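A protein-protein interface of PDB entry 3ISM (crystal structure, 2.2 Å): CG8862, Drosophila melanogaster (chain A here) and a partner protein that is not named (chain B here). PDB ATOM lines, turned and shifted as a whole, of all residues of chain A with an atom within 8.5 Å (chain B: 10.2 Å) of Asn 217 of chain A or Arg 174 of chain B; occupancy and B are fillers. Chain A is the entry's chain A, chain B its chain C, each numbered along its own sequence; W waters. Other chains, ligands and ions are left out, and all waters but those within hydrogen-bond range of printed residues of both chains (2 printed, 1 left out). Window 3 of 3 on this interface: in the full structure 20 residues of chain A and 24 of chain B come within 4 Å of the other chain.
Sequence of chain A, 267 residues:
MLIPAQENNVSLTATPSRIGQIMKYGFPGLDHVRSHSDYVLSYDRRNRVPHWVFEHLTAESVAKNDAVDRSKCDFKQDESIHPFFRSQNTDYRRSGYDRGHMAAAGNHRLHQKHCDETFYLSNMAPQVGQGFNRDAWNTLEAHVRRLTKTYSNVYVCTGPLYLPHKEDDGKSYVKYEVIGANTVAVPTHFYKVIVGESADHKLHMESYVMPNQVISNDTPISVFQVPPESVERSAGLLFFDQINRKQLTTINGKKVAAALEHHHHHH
NE2 of Gln 130 of chain A lies within hydrogen-bond range of O of Arg 142 of chain B, at 3.2 Å. O of Ser 141 of chain B lies close to NH2 of Arg 134 of chain A, at 2.9 Å. The guanidinium group (NH2) of Arg 134 of chain A is in hydrogen-bond range of the backbone carbonyl oxygen (O) of Arg 142 of chain B, 3.1 Å away. The backbone carbonyl oxygen (O) of Arg 134 of chain A is in hydrogen-bond range of the backbone NH (N) of Ser 149 of chain B, at 2.9 Å.
O of Gly 129 of chain A lies within hydrogen-bond range of N of Arg 134 of chain A, at 3.0 Å. OD2 of Asp 135 of chain A sits at hydrogen-bond distance from N of Gly 131 of chain A (2.8 Å). The backbone carbonyl oxygen of Asp 135 of chain A sits at hydrogen-bond distance from the side-chain hydroxyl of Thr 139 of chain A. The guanidinium group (NH2) of Arg 142 of chain B sits at hydrogen-bond distance from the side-chain hydroxyl (OG) of Ser 170 of chain B (3.3 Å). The side-chain carboxylate of Asp 148 of chain B sits at hydrogen-bond distance from the backbone NH of Asp 150 of chain B (2.9 Å). The backbone carbonyl oxygen of Ser 170 of chain B lies close to the guanidinium group of Arg 174 of chain B (3.3 Å).
Among the printed residues, merely in contact across the chains: Arg 134 of chain A with Asp 148 of chain B, Asp 135 of chain A with Ser 149 of chain B and Asn 217 of chain A with Arg 174 of chain B.
No residue of chain B comes within 4 Å of Gly 131 of chain A. Printed residues of chain B within 4 Å of Arg 134 of chain A: Ser 141 (2.9 Å), Arg 142 (3.1 Å), Asp 148 (3.7 Å) and Ser 149 (2.9 Å). Asp 135 of chain A touches just one residue of chain B: Ser 149 (3.7 Å). No residue of chain B comes within 4 Å of Ser 216 of chain A. Asn 217 of chain A touches one residue of chain B. No residue of chain B comes within 4 Å of Asp 218 of chain A. Thr 219 of chain A touches none of the printed residues of chain B. Of the printed residues of chain A, Asp 148 of chain B touches Arg 134. Ala 169 of chain B touches none of the printed residues of chain A. Arg 174 of chain B touches just one residue of chain A: Asn 217. The nearest residue of chain B that does not touch Asn 217 of chain A is Ser 149 of chain B (6.5 Å). The nearest residue of chain A that does not touch Arg 174 of chain B is Asp 218 of chain A (6.4 Å). The nearest printed residue of chain A that does not touch Arg 142 of chain B is Asp 135 of chain A (6.9 Å).
Of the 17 printed residues of chain A, 4 touch a printed residue of chain B. Along chain A the printed residues that touch a printed residue of chain B span positions 130 to 217. Among the printed residues, 7 pairs touch across the chains. Among the printed residues, no Asp or Glu carboxylate lies within 4 Å of a Lys or Arg side-chain nitrogen of the other chain.
Water W2 bridges OG of Ser 141 of chain B and OD1 of Asp 135 of chain A. Water W1 bridges the side-chain carboxylate (OD2) of Asp 135 of chain A (2.8 Å) and the backbone carbonyl oxygen (O) of Ser 141 of chain B (3.1 Å).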
ATOM      1  N   GLY A 129     -11.222 -11.277   3.442  1.00  0.00           N
ATOM      2  CA  GLY A 129      -9.991 -11.403   2.661  1.00  0.00           C
ATOM      3  C   GLY A 129      -9.360 -10.100   2.218  1.00  0.00           C
ATOM      4  O   GLY A 129      -8.502  -9.537   2.927  1.00  0.00           O
ATOM      5  N   GLN A 130      -9.754  -9.637   1.034  1.00  0.00           N
ATOM      6  CA  GLN A 130      -9.319  -8.348   0.534  1.00  0.00           C
ATOM      7  C   GLN A 130      -9.836  -7.275   1.493  1.00  0.00           C
ATOM      8  O   GLN A 130     -10.980  -7.320   1.923  1.00  0.00           O
ATOM      9  CB  GLN A 130      -9.900  -8.061  -0.864  1.00  0.00           C
ATOM     10  CG  GLN A 130      -9.354  -8.885  -1.989  1.00  0.00           C
ATOM     11  CD  GLN A 130     -10.043  -8.528  -3.308  1.00  0.00           C
ATOM     12  OE1 GLN A 130      -9.714  -7.514  -3.947  1.00  0.00           O
ATOM     13  NE2 GLN A 130     -11.025  -9.339  -3.699  1.00  0.00           N
ATOM     14  N   GLY A 131      -8.989  -6.317   1.825  1.00  0.00           N
ATOM     15  CA  GLY A 131      -9.416  -5.222   2.687  1.00  0.00           C
ATOM     16  C   GLY A 131      -9.261  -5.580   4.148  1.00  0.00           C
ATOM     17  O   GLY A 131      -9.521  -4.745   5.014  1.00  0.00           O
ATOM     18  N   PHE A 132      -8.832  -6.811   4.430  1.00  0.00           N
ATOM     19  CA  PHE A 132      -8.620  -7.235   5.814  1.00  0.00           C
ATOM     20  C   PHE A 132      -7.471  -8.240   6.026  1.00  0.00           C
ATOM     21  O   PHE A 132      -6.338  -7.816   6.218  1.00  0.00           O
ATOM     22  CB  PHE A 132      -9.916  -7.670   6.524  1.00  0.00           C
ATOM     23  CG  PHE A 132      -9.745  -7.835   8.020  1.00  0.00           C
ATOM     24  CD1 PHE A 132      -9.397  -6.739   8.823  1.00  0.00           C
ATOM     25  CD2 PHE A 132      -9.904  -9.084   8.625  1.00  0.00           C
ATOM     26  CE1 PHE A 132      -9.213  -6.891  10.209  1.00  0.00           C
ATOM     27  CE2 PHE A 132      -9.725  -9.237   9.994  1.00  0.00           C
ATOM     28  CZ  PHE A 132      -9.383  -8.140  10.788  1.00  0.00           C
ATOM     29  N   ARG A 134      -5.712 -10.028   3.984  1.00  0.00           N
ATOM     30  CA  ARG A 134      -4.660  -9.869   2.991  1.00  0.00           C
ATOM     31  C   ARG A 134      -4.033  -8.471   3.001  1.00  0.00           C
ATOM     32  O   ARG A 134      -2.986  -8.231   2.384  1.00  0.00           O
ATOM     33  CB  ARG A 134      -5.248 -10.193   1.622  1.00  0.00           C
ATOM     34  CG  ARG A 134      -5.842 -11.608   1.570  1.00  0.00           C
ATOM     35  CD  ARG A 134      -6.450 -11.891   0.221  1.00  0.00           C
ATOM     36  NE  ARG A 134      -7.561 -12.835   0.290  1.00  0.00           N
ATOM     37  CZ  ARG A 134      -8.411 -13.059  -0.703  1.00  0.00           C
ATOM     38  NH1 ARG A 134      -9.404 -13.930  -0.529  1.00  0.00           N
ATOM     39  NH2 ARG A 134      -8.276 -12.421  -1.866  1.00  0.00           N
ATOM     40  N   ASP A 135      -4.674  -7.553   3.721  1.00  0.00           N
ATOM     41  CA  ASP A 135      -4.318  -6.145   3.649  1.00  0.00           C
ATOM     42  C   ASP A 135      -4.164  -5.565   5.060  1.00  0.00           C
ATOM     43  O   ASP A 135      -3.127  -5.801   5.710  1.00  0.00           O
ATOM     44  CB  ASP A 135      -5.356  -5.402   2.799  1.00  0.00           C
ATOM     45  CG  ASP A 135      -5.325  -5.834   1.311  1.00  0.00           C
ATOM     46  OD1 ASP A 135      -4.279  -5.617   0.644  1.00  0.00           O
ATOM     47  OD2 ASP A 135      -6.334  -6.379   0.801  1.00  0.00           O
ATOM     48  N   ALA A 136      -5.180  -4.850   5.552  1.00  0.00           N
ATOM     49  CA  ALA A 136      -5.096  -4.120   6.852  1.00  0.00           C
ATOM     50  C   ALA A 136      -4.610  -4.959   8.056  1.00  0.00           C
ATOM     51  O   ALA A 136      -3.819  -4.502   8.869  1.00  0.00           O
ATOM     52  CB  ALA A 136      -6.430  -3.476   7.182  1.00  0.00           C
ATOM     53  N   TRP A 137      -5.109  -6.185   8.170  1.00  0.00           N
ATOM     54  CA  TRP A 137      -4.665  -7.099   9.229  1.00  0.00           C
ATOM     55  C   TRP A 137      -3.193  -7.517   9.028  1.00  0.00           C
ATOM     56  O   TRP A 137      -2.401  -7.578   9.985  1.00  0.00           O
ATOM     57  CB  TRP A 137      -5.611  -8.323   9.305  1.00  0.00           C
ATOM     58  CG  TRP A 137      -5.318  -9.210  10.469  1.00  0.00           C
ATOM     59  CD1 TRP A 137      -4.736 -10.443  10.439  1.00  0.00           C
ATOM     60  CD2 TRP A 137      -5.559  -8.909  11.858  1.00  0.00           C
ATOM     61  NE1 TRP A 137      -4.567 -10.925  11.735  1.00  0.00           N
ATOM     62  CE2 TRP A 137      -5.097 -10.014  12.615  1.00  0.00           C
ATOM     63  CE3 TRP A 137      -6.112  -7.816  12.532  1.00  0.00           C
ATOM     64  CZ2 TRP A 137      -5.175 -10.052  14.014  1.00  0.00           C
ATOM     65  CZ3 TRP A 137      -6.189  -7.860  13.947  1.00  0.00           C
ATOM     66  CH2 TRP A 137      -5.720  -8.967  14.657  1.00  0.00           C
ATOM     67  N   THR A 139      -1.062  -5.551   7.534  1.00  0.00           N
ATOM     68  CA  THR A 139      -0.362  -4.328   7.938  1.00  0.00           C
ATOM     69  C   THR A 139      -0.073  -4.297   9.446  1.00  0.00           C
ATOM     70  O   THR A 139       1.040  -3.948   9.862  1.00  0.00           O
ATOM     71  CB  THR A 139      -1.160  -3.060   7.524  1.00  0.00           C
ATOM     72  OG1 THR A 139      -1.408  -3.104   6.110  1.00  0.00           O
ATOM     73  CG2 THR A 139      -0.405  -1.770   7.897  1.00  0.00           C
ATOM     74  N   VAL A 214     -13.958  -5.113   5.511  1.00  0.00           N
ATOM     75  CA  VAL A 214     -13.096  -4.397   4.596  1.00  0.00           C
ATOM     76  C   VAL A 214     -12.693  -3.076   5.246  1.00  0.00           C
ATOM     77  O   VAL A 214     -13.548  -2.281   5.677  1.00  0.00           O
ATOM     78  CB  VAL A 214     -13.798  -4.155   3.226  1.00  0.00           C
ATOM     79  CG1 VAL A 214     -12.973  -3.237   2.338  1.00  0.00           C
ATOM     80  CG2 VAL A 214     -14.059  -5.498   2.517  1.00  0.00           C
ATOM     81  N   ILE A 215     -11.381  -2.870   5.346  1.00  0.00           N
ATOM     82  CA  ILE A 215     -10.824  -1.625   5.865  1.00  0.00           C
ATOM     83  C   ILE A 215      -9.992  -1.019   4.739  1.00  0.00           C
ATOM     84  O   ILE A 215      -9.227  -1.726   4.071  1.00  0.00           O
ATOM     85  CB  ILE A 215      -9.966  -1.882   7.139  1.00  0.00           C
ATOM     86  CG1 ILE A 215     -10.790  -2.587   8.218  1.00  0.00           C
ATOM     87  CG2 ILE A 215      -9.380  -0.585   7.722  1.00  0.00           C
ATOM     88  CD1 ILE A 215      -9.915  -3.138   9.355  1.00  0.00           C
ATOM     89  N   SER A 216     -10.192   0.274   4.492  1.00  0.00           N
ATOM     90  CA  SER A 216      -9.385   1.039   3.549  1.00  0.00           C
ATOM     91  C   SER A 216      -7.886   0.874   3.804  1.00  0.00           C
ATOM     92  O   SER A 216      -7.435   0.912   4.959  1.00  0.00           O
ATOM     93  CB  SER A 216      -9.751   2.517   3.657  1.00  0.00           C
ATOM     94  OG  SER A 216      -8.837   3.307   2.921  1.00  0.00           O
ATOM     95  N   ASN A 217      -7.119   0.707   2.725  1.00  0.00           N
ATOM     96  CA  ASN A 217      -5.648   0.691   2.796  1.00  0.00           C
ATOM     97  C   ASN A 217      -5.056   2.023   3.270  1.00  0.00           C
ATOM     98  O   ASN A 217      -3.896   2.086   3.678  1.00  0.00           O
ATOM     99  CB  ASN A 217      -5.048   0.315   1.425  1.00  0.00           C
ATOM    100  CG  ASN A 217      -5.355  -1.127   1.021  1.00  0.00           C
ATOM    101  OD1 ASN A 217      -5.416  -2.015   1.860  1.00  0.00           O
ATOM    102  ND2 ASN A 217      -5.561  -1.353  -0.274  1.00  0.00           N
ATOM    103  N   ASP A 218      -5.850   3.087   3.192  1.00  0.00           N
ATOM    104  CA  ASP A 218      -5.462   4.409   3.699  1.00  0.00           C
ATOM    105  C   ASP A 218      -5.506   4.539   5.216  1.00  0.00           C
ATOM    106  O   ASP A 218      -4.874   5.437   5.770  1.00  0.00           O
ATOM    107  CB  ASP A 218      -6.420   5.480   3.175  1.00  0.00           C
ATOM    108  CG  ASP A 218      -6.088   5.933   1.795  1.00  0.00           C
ATOM    109  OD1 ASP A 218      -5.186   5.342   1.160  1.00  0.00           O
ATOM    110  OD2 ASP A 218      -6.739   6.891   1.347  1.00  0.00           O
ATOM    111  N   THR A 219      -6.302   3.701   5.871  1.00  0.00           N
ATOM    112  CA  THR A 219      -6.531   3.834   7.298  1.00  0.00           C
ATOM    113  C   THR A 219      -5.288   3.470   8.107  1.00  0.00           C
ATOM    114  O   THR A 219      -4.851   2.328   8.087  1.00  0.00           O
ATOM    115  CB  THR A 219      -7.720   2.960   7.756  1.00  0.00           C
ATOM    116  OG1 THR A 219      -8.889   3.341   7.015  1.00  0.00           O
ATOM    117  CG2 THR A 219      -7.975   3.148   9.265  1.00  0.00           C
ATOM    118  N   PRO A 220      -4.733   4.444   8.848  1.00  0.00           N
ATOM    119  CA  PRO A 220      -3.578   4.147   9.696  1.00  0.00           C
ATOM    120  C   PRO A 220      -4.011   3.176  10.788  1.00  0.00           C
ATOM    121  O   PRO A 220      -5.120   3.311  11.308  1.00  0.00           O
ATOM    122  CB  PRO A 220      -3.216   5.516  10.308  1.00  0.00           C
ATOM    123  CG  PRO A 220      -3.937   6.541   9.469  1.00  0.00           C
ATOM    124  CD  PRO A 220      -5.167   5.848   8.967  1.00  0.00           C
ATOM    125  N   ILE A 221      -3.166   2.206  11.133  1.00  0.00           N
ATOM    126  CA  ILE A 221      -3.560   1.221  12.143  1.00  0.00           C
ATOM    127  C   ILE A 221      -3.681   1.811  13.549  1.00  0.00           C
ATOM    128  O   ILE A 221      -4.288   1.194  14.410  1.00  0.00           O
ATOM    129  CB  ILE A 221      -2.613  -0.021  12.190  1.00  0.00           C
ATOM    130  CG1 ILE A 221      -1.187   0.422  12.525  1.00  0.00           C
ATOM    131  CG2 ILE A 221      -2.673  -0.800  10.878  1.00  0.00           C
ATOM    132  CD1 ILE A 221      -0.258  -0.723  12.834  1.00  0.00           C
ATOM    133  N   TRP B 140      -2.914 -14.706  -6.747  1.00  0.00           N
ATOM    134  CA  TRP B 140      -2.210 -13.765  -5.865  1.00  0.00           C
ATOM    135  C   TRP B 140      -3.146 -13.200  -4.787  1.00  0.00           C
ATOM    136  O   TRP B 140      -4.246 -13.715  -4.605  1.00  0.00           O
ATOM    137  CB  TRP B 140      -1.536 -12.637  -6.670  1.00  0.00           C
ATOM    138  CG  TRP B 140      -2.431 -11.657  -7.372  1.00  0.00           C
ATOM    139  CD1 TRP B 140      -3.314 -11.926  -8.378  1.00  0.00           C
ATOM    140  CD2 TRP B 140      -2.470 -10.233  -7.178  1.00  0.00           C
ATOM    141  NE1 TRP B 140      -3.917 -10.762  -8.806  1.00  0.00           N
ATOM    142  CE2 TRP B 140      -3.406  -9.708  -8.093  1.00  0.00           C
ATOM    143  CE3 TRP B 140      -1.808  -9.351  -6.309  1.00  0.00           C
ATOM    144  CZ2 TRP B 140      -3.711  -8.339  -8.157  1.00  0.00           C
ATOM    145  CZ3 TRP B 140      -2.108  -8.004  -6.368  1.00  0.00           C
ATOM    146  CH2 TRP B 140      -3.051  -7.507  -7.288  1.00  0.00           C
ATOM    147  N   SER B 141      -2.743 -12.137  -4.088  1.00  0.00           N
ATOM    148  CA  SER B 141      -3.568 -11.671  -2.957  1.00  0.00           C
ATOM    149  C   SER B 141      -4.948 -11.104  -3.331  1.00  0.00           C
ATOM    150  O   SER B 141      -5.812 -10.946  -2.469  1.00  0.00           O
ATOM    151  CB  SER B 141      -2.802 -10.708  -2.039  1.00  0.00           C
ATOM    152  OG  SER B 141      -2.441  -9.531  -2.722  1.00  0.00           O
ATOM    153  N   ARG B 142      -5.156 -10.809  -4.608  1.00  0.00           N
ATOM    154  CA  ARG B 142      -6.456 -10.322  -5.047  1.00  0.00           C
ATOM    155  C   ARG B 142      -7.487 -11.442  -4.960  1.00  0.00           C
ATOM    156  O   ARG B 142      -8.651 -11.190  -4.651  1.00  0.00           O
ATOM    157  CB  ARG B 142      -6.367  -9.777  -6.475  1.00  0.00           C
ATOM    158  CG  ARG B 142      -7.552  -8.949  -6.957  1.00  0.00           C
ATOM    159  CD  ARG B 142      -7.761  -7.671  -6.168  1.00  0.00           C
ATOM    160  NE  ARG B 142      -6.588  -6.800  -6.096  1.00  0.00           N
ATOM    161  CZ  ARG B 142      -6.335  -5.794  -6.931  1.00  0.00           C
ATOM    162  NH1 ARG B 142      -7.165  -5.527  -7.939  1.00  0.00           N
ATOM    163  NH2 ARG B 142      -5.244  -5.057  -6.763  1.00  0.00           N
ATOM    164  N   ASP B 148      -0.761 -12.462   0.411  1.00  0.00           N
ATOM    165  CA  ASP B 148      -1.070 -11.193   1.091  1.00  0.00           C
ATOM    166  C   ASP B 148      -0.390 -10.009   0.374  1.00  0.00           C
ATOM    167  O   ASP B 148       0.279 -10.198  -0.647  1.00  0.00           O
ATOM    168  CB  ASP B 148      -0.697 -11.234   2.579  1.00  0.00           C
ATOM    169  CG  ASP B 148       0.815 -11.401   2.818  1.00  0.00           C
ATOM    170  OD1 ASP B 148       1.175 -12.125   3.772  1.00  0.00           O
ATOM    171  OD2 ASP B 148       1.634 -10.826   2.067  1.00  0.00           O
ATOM    172  N   SER B 149      -0.555  -8.813   0.925  1.00  0.00           N
ATOM    173  CA  SER B 149      -0.096  -7.581   0.285  1.00  0.00           C
ATOM    174  C   SER B 149       1.426  -7.414   0.184  1.00  0.00           C
ATOM    175  O   SER B 149       1.897  -6.546  -0.562  1.00  0.00           O
ATOM    176  CB  SER B 149      -0.672  -6.360   1.018  1.00  0.00           C
ATOM    177  OG  SER B 149      -0.219  -6.320   2.370  1.00  0.00           O
ATOM    178  N   ASP B 150       2.184  -8.206   0.950  1.00  0.00           N
ATOM    179  CA  ASP B 150       3.652  -8.132   0.893  1.00  0.00           C
ATOM    180  C   ASP B 150       4.237  -9.034  -0.193  1.00  0.00           C
ATOM    181  O   ASP B 150       5.411  -8.919  -0.526  1.00  0.00           O
ATOM    182  CB  ASP B 150       4.294  -8.421   2.258  1.00  0.00           C
ATOM    183  CG  ASP B 150       4.000  -7.339   3.282  1.00  0.00           C
ATOM    184  OD1 ASP B 150       3.892  -6.157   2.885  1.00  0.00           O
ATOM    185  OD2 ASP B 150       3.874  -7.666   4.485  1.00  0.00           O
ATOM    186  N   PRO B 153       2.917  -8.909  -6.712  1.00  0.00           N
ATOM    187  CA  PRO B 153       1.813  -9.108  -7.666  1.00  0.00           C
ATOM    188  C   PRO B 153       2.331  -9.539  -9.041  1.00  0.00           C
ATOM    189  O   PRO B 153       3.426  -9.123  -9.425  1.00  0.00           O
ATOM    190  CB  PRO B 153       1.154  -7.732  -7.748  1.00  0.00           C
ATOM    191  CG  PRO B 153       2.172  -6.760  -7.217  1.00  0.00           C
ATOM    192  CD  PRO B 153       3.028  -7.508  -6.255  1.00  0.00           C
ATOM    193  N   PRO B 166      -4.959  -5.706 -15.883  1.00  0.00           N
ATOM    194  CA  PRO B 166      -6.113  -4.824 -15.637  1.00  0.00           C
ATOM    195  C   PRO B 166      -6.039  -4.146 -14.270  1.00  0.00           C
ATOM    196  O   PRO B 166      -6.581  -3.053 -14.100  1.00  0.00           O
ATOM    197  CB  PRO B 166      -7.306  -5.779 -15.665  1.00  0.00           C
ATOM    198  CG  PRO B 166      -6.833  -6.944 -16.430  1.00  0.00           C
ATOM    199  CD  PRO B 166      -5.384  -7.094 -16.122  1.00  0.00           C
ATOM    200  N   PHE B 167      -5.351  -4.787 -13.324  1.00  0.00           N
ATOM    201  CA  PHE B 167      -5.134  -4.215 -12.002  1.00  0.00           C
ATOM    202  C   PHE B 167      -3.896  -3.318 -11.876  1.00  0.00           C
ATOM    203  O   PHE B 167      -3.593  -2.827 -10.777  1.00  0.00           O
ATOM    204  CB  PHE B 167      -5.055  -5.322 -10.959  1.00  0.00           C
ATOM    205  CG  PHE B 167      -3.970  -6.332 -11.215  1.00  0.00           C
ATOM    206  CD1 PHE B 167      -4.281  -7.582 -11.710  1.00  0.00           C
ATOM    207  CD2 PHE B 167      -2.641  -6.043 -10.935  1.00  0.00           C
ATOM    208  CE1 PHE B 167      -3.285  -8.521 -11.937  1.00  0.00           C
ATOM    209  CE2 PHE B 167      -1.641  -6.979 -11.161  1.00  0.00           C
ATOM    210  CZ  PHE B 167      -1.965  -8.223 -11.654  1.00  0.00           C
ATOM    211  N   ALA B 168      -3.168  -3.114 -12.972  1.00  0.00           N
ATOM    212  CA  ALA B 168      -1.917  -2.340 -12.912  1.00  0.00           C
ATOM    213  C   ALA B 168      -2.116  -0.942 -12.329  1.00  0.00           C
ATOM    214  O   ALA B 168      -1.354  -0.524 -11.452  1.00  0.00           O
ATOM    215  CB  ALA B 168      -1.243  -2.266 -14.273  1.00  0.00           C
ATOM    216  N   ALA B 169      -3.142  -0.236 -12.807  1.00  0.00           N
ATOM    217  CA  ALA B 169      -3.431   1.128 -12.338  1.00  0.00           C
ATOM    218  C   ALA B 169      -3.729   1.174 -10.845  1.00  0.00           C
ATOM    219  O   ALA B 169      -3.281   2.093 -10.160  1.00  0.00           O
ATOM    220  CB  ALA B 169      -4.573   1.747 -13.133  1.00  0.00           C
ATOM    221  N   SER B 170      -4.467   0.170 -10.355  1.00  0.00           N
ATOM    222  CA  SER B 170      -4.799   0.041  -8.928  1.00  0.00           C
ATOM    223  C   SER B 170      -3.567  -0.097  -8.038  1.00  0.00           C
ATOM    224  O   SER B 170      -3.525   0.490  -6.958  1.00  0.00           O
ATOM    225  CB  SER B 170      -5.767  -1.127  -8.668  1.00  0.00           C
ATOM    226  OG  SER B 170      -5.112  -2.399  -8.660  1.00  0.00           O
ATOM    227  N   LEU B 171      -2.569  -0.852  -8.489  1.00  0.00           N
ATOM    228  CA  LEU B 171      -1.339  -1.040  -7.709  1.00  0.00           C
ATOM    229  C   LEU B 171      -0.479   0.208  -7.569  1.00  0.00           C
ATOM    230  O   LEU B 171       0.135   0.414  -6.517  1.00  0.00           O
ATOM    231  CB  LEU B 171      -0.493  -2.166  -8.278  1.00  0.00           C
ATOM    232  CG  LEU B 171      -1.059  -3.557  -8.041  1.00  0.00           C
ATOM    233  CD1 LEU B 171      -0.165  -4.553  -8.732  1.00  0.00           C
ATOM    234  CD2 LEU B 171      -1.196  -3.848  -6.535  1.00  0.00           C
ATOM    235  N   LYS B 172      -0.420   1.023  -8.626  1.00  0.00           N
ATOM    236  CA  LYS B 172       0.340   2.274  -8.575  1.00  0.00           C
ATOM    237  C   LYS B 172      -0.245   3.210  -7.525  1.00  0.00           C
ATOM    238  O   LYS B 172       0.499   3.868  -6.800  1.00  0.00           O
ATOM    239  CB  LYS B 172       0.410   2.960  -9.948  1.00  0.00           C
ATOM    240  CG  LYS B 172       1.278   2.223 -10.955  1.00  0.00           C
ATOM    241  CD  LYS B 172       1.140   2.786 -12.361  1.00  0.00           C
ATOM    242  CE  LYS B 172       1.503   1.725 -13.398  1.00  0.00           C
ATOM    243  NZ  LYS B 172       1.708   2.287 -14.761  1.00  0.00           N
ATOM    244  N   VAL B 173      -1.574   3.236  -7.427  1.00  0.00           N
ATOM    245  CA  VAL B 173      -2.265   4.077  -6.444  1.00  0.00           C
ATOM    246  C   VAL B 173      -2.131   3.527  -5.012  1.00  0.00           C
ATOM    247  O   VAL B 173      -2.022   4.306  -4.068  1.00  0.00           O
ATOM    248  CB  VAL B 173      -3.750   4.366  -6.846  1.00  0.00           C
ATOM    249  CG1 VAL B 173      -4.405   5.349  -5.885  1.00  0.00           C
ATOM    250  CG2 VAL B 173      -3.818   4.944  -8.253  1.00  0.00           C
ATOM    251  N   ARG B 174      -2.101   2.205  -4.848  1.00  0.00           N
ATOM    252  CA  ARG B 174      -1.941   1.616  -3.506  1.00  0.00           C
ATOM    253  C   ARG B 174      -0.567   1.930  -2.898  1.00  0.00           C
ATOM    254  O   ARG B 174       0.476   1.614  -3.479  1.00  0.00           O
ATOM    255  CB  ARG B 174      -2.181   0.092  -3.495  1.00  0.00           C
ATOM    256  CG  ARG B 174      -3.490  -0.413  -4.134  1.00  0.00           C
ATOM    257  CD  ARG B 174      -4.764   0.241  -3.589  1.00  0.00           C
ATOM    258  NE  ARG B 174      -5.806   0.321  -4.621  1.00  0.00           N
ATOM    259  CZ  ARG B 174      -6.370   1.453  -5.048  1.00  0.00           C
ATOM    260  NH1 ARG B 174      -6.022   2.621  -4.518  1.00  0.00           N
ATOM    261  NH2 ARG B 174      -7.300   1.416  -5.996  1.00  0.00           N
HETATM  262  O   HOH W   1      -6.104  -8.025  -1.459  1.00  0.00           O
HETATM  263  O   HOH W   2      -3.075  -7.379  -1.298  1.00  0.00           O
